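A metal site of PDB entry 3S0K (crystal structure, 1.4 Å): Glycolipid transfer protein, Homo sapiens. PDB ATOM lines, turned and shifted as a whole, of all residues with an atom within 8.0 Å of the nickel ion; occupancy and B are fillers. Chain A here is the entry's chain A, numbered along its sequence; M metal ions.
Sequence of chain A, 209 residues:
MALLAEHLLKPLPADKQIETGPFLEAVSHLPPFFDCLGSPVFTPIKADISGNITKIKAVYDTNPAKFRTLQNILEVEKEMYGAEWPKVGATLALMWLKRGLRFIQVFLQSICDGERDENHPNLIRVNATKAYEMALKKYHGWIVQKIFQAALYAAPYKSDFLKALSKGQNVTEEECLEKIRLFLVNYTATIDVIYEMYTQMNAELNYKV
The backbone carbonyl oxygen (O) of Glu 25 sits at hydrogen-bond distance from the side-chain hydroxyl (OG) of Ser 28, at 2.7 Å.
The nearest printed residue that does not touch the nickel ion is Ala 26 (4.7 Å).
NE2 of His 29 binds the nickel ion (2.1 Å). The nickel ion is bound by a ring nitrogen (NE2) of His 7 (2.1 Å). The nickel ion is bound by OE1 of Glu 25 (2.1 Å). The nickel ion is bound by OE2 of Glu 25 (2.5 Å). The nickel ion has four donor atoms within binding distance.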
ATOM      1  N   HIS A   7       4.246 -29.779  -1.588  1.00  0.00           N
ATOM      2  CA  HIS A   7       2.789 -29.953  -1.882  1.00  0.00           C
ATOM      3  C   HIS A   7       2.454 -30.761  -3.139  1.00  0.00           C
ATOM      4  O   HIS A   7       3.198 -30.861  -4.064  1.00  0.00           O
ATOM      5  CB  HIS A   7       2.065 -28.612  -1.924  1.00  0.00           C
ATOM      6  CG  HIS A   7       2.310 -27.742  -3.133  1.00  0.00           C
ATOM      7  ND1 HIS A   7       1.521 -27.810  -4.273  1.00  0.00           N
ATOM      8  CD2 HIS A   7       3.137 -26.692  -3.325  1.00  0.00           C
ATOM      9  CE1 HIS A   7       1.881 -26.855  -5.116  1.00  0.00           C
ATOM     10  NE2 HIS A   7       2.863 -26.164  -4.561  1.00  0.00           N
ATOM     11  N   LEU A   8       1.256 -31.277  -3.117  1.00  0.00           N
ATOM     12  CA  LEU A   8       0.669 -32.085  -4.217  1.00  0.00           C
ATOM     13  C   LEU A   8       0.014 -31.155  -5.227  1.00  0.00           C
ATOM     14  O   LEU A   8      -0.225 -29.998  -4.915  1.00  0.00           O
ATOM     15  CB  LEU A   8      -0.427 -33.021  -3.631  1.00  0.00           C
ATOM     16  CG  LEU A   8       0.093 -33.992  -2.583  1.00  0.00           C
ATOM     17  CD1 LEU A   8      -1.008 -34.860  -1.955  1.00  0.00           C
ATOM     18  CD2 LEU A   8       1.135 -34.884  -3.229  1.00  0.00           C
ATOM     19  N   PRO A  22      -3.014 -22.645 -10.712  1.00  0.00           N
ATOM     20  CA  PRO A  22      -2.483 -23.659  -9.823  1.00  0.00           C
ATOM     21  C   PRO A  22      -1.657 -24.693 -10.557  1.00  0.00           C
ATOM     22  O   PRO A  22      -0.678 -25.211 -10.019  1.00  0.00           O
ATOM     23  CB  PRO A  22      -3.739 -24.224  -9.142  1.00  0.00           C
ATOM     24  CG  PRO A  22      -4.709 -23.053  -9.187  1.00  0.00           C
ATOM     25  CD  PRO A  22      -4.471 -22.446 -10.556  1.00  0.00           C
ATOM     26  N   LEU A  24       0.152 -24.270 -13.321  1.00  0.00           N
ATOM     27  CA  LEU A  24       1.491 -23.693 -13.656  1.00  0.00           C
ATOM     28  C   LEU A  24       2.337 -23.515 -12.432  1.00  0.00           C
ATOM     29  O   LEU A  24       3.523 -23.772 -12.457  1.00  0.00           O
ATOM     30  CB  LEU A  24       1.340 -22.351 -14.339  1.00  0.00           C
ATOM     31  CG  LEU A  24       0.680 -22.437 -15.707  1.00  0.00           C
ATOM     32  CD1 LEU A  24       0.448 -21.044 -16.222  1.00  0.00           C
ATOM     33  CD2 LEU A  24       1.508 -23.287 -16.713  1.00  0.00           C
ATOM     34  N   GLU A  25       1.720 -23.136 -11.335  1.00  0.00           N
ATOM     35  CA  GLU A  25       2.494 -22.951 -10.125  1.00  0.00           C
ATOM     36  C   GLU A  25       3.079 -24.285  -9.661  1.00  0.00           C
ATOM     37  O   GLU A  25       4.244 -24.378  -9.303  1.00  0.00           O
ATOM     38  CB  GLU A  25       1.634 -22.324  -9.063  1.00  0.00           C
ATOM     39  CG  GLU A  25       2.397 -21.608  -7.936  1.00  0.00           C
ATOM     40  CD  GLU A  25       3.061 -22.566  -6.986  1.00  0.00           C
ATOM     41  OE1 GLU A  25       2.451 -23.625  -6.703  1.00  0.00           O
ATOM     42  OE2 GLU A  25       4.198 -22.255  -6.512  1.00  0.00           O
ATOM     43  N   ALA A  26       2.299 -25.342  -9.727  1.00  0.00           N
ATOM     44  CA  ALA A  26       2.774 -26.631  -9.281  1.00  0.00           C
ATOM     45  C   ALA A  26       3.876 -27.168 -10.186  1.00  0.00           C
ATOM     46  O   ALA A  26       4.912 -27.658  -9.713  1.00  0.00           O
ATOM     47  CB  ALA A  26       1.597 -27.619  -9.217  1.00  0.00           C
ATOM     48  N   VAL A  27       3.675 -27.103 -11.495  1.00  0.00           N
ATOM     49  CA  VAL A  27       4.682 -27.687 -12.375  1.00  0.00           C
ATOM     50  C   VAL A  27       5.935 -26.860 -12.437  1.00  0.00           C
ATOM     51  O   VAL A  27       7.008 -27.374 -12.793  1.00  0.00           O
ATOM     52  CB  VAL A  27       4.150 -28.042 -13.784  1.00  0.00           C
ATOM     53  CG1 VAL A  27       2.989 -29.045 -13.650  1.00  0.00           C
ATOM     54  CG2 VAL A  27       3.741 -26.825 -14.550  1.00  0.00           C
ATOM     55  N   SER A  28       5.845 -25.607 -11.993  1.00  0.00           N
ATOM     56  CA  SER A  28       7.025 -24.733 -11.892  1.00  0.00           C
ATOM     57  C   SER A  28       8.047 -25.239 -10.863  1.00  0.00           C
ATOM     58  O   SER A  28       9.222 -24.875 -10.879  1.00  0.00           O
ATOM     59  CB  SER A  28       6.594 -23.304 -11.594  1.00  0.00           C
ATOM     60  OG  SER A  28       6.473 -23.179 -10.176  1.00  0.00           O
ATOM     61  N   HIS A  29       7.627 -26.126  -9.980  1.00  0.00           N
ATOM     62  CA  HIS A  29       8.551 -26.725  -9.031  1.00  0.00           C
ATOM     63  C   HIS A  29       9.349 -27.860  -9.613  1.00  0.00           C
ATOM     64  O   HIS A  29      10.256 -28.376  -8.922  1.00  0.00           O
ATOM     65  CB  HIS A  29       7.805 -27.250  -7.820  1.00  0.00           C
ATOM     66  CG  HIS A  29       7.075 -26.201  -7.071  1.00  0.00           C
ATOM     67  ND1 HIS A  29       7.674 -25.036  -6.666  1.00  0.00           N
ATOM     68  CD2 HIS A  29       5.792 -26.137  -6.609  1.00  0.00           C
ATOM     69  CE1 HIS A  29       6.792 -24.295  -5.997  1.00  0.00           C
ATOM     70  NE2 HIS A  29       5.648 -24.951  -5.943  1.00  0.00           N
HETATM   71 NI    NI M   1       3.795 -24.396  -5.226  1.00  0.00          NI
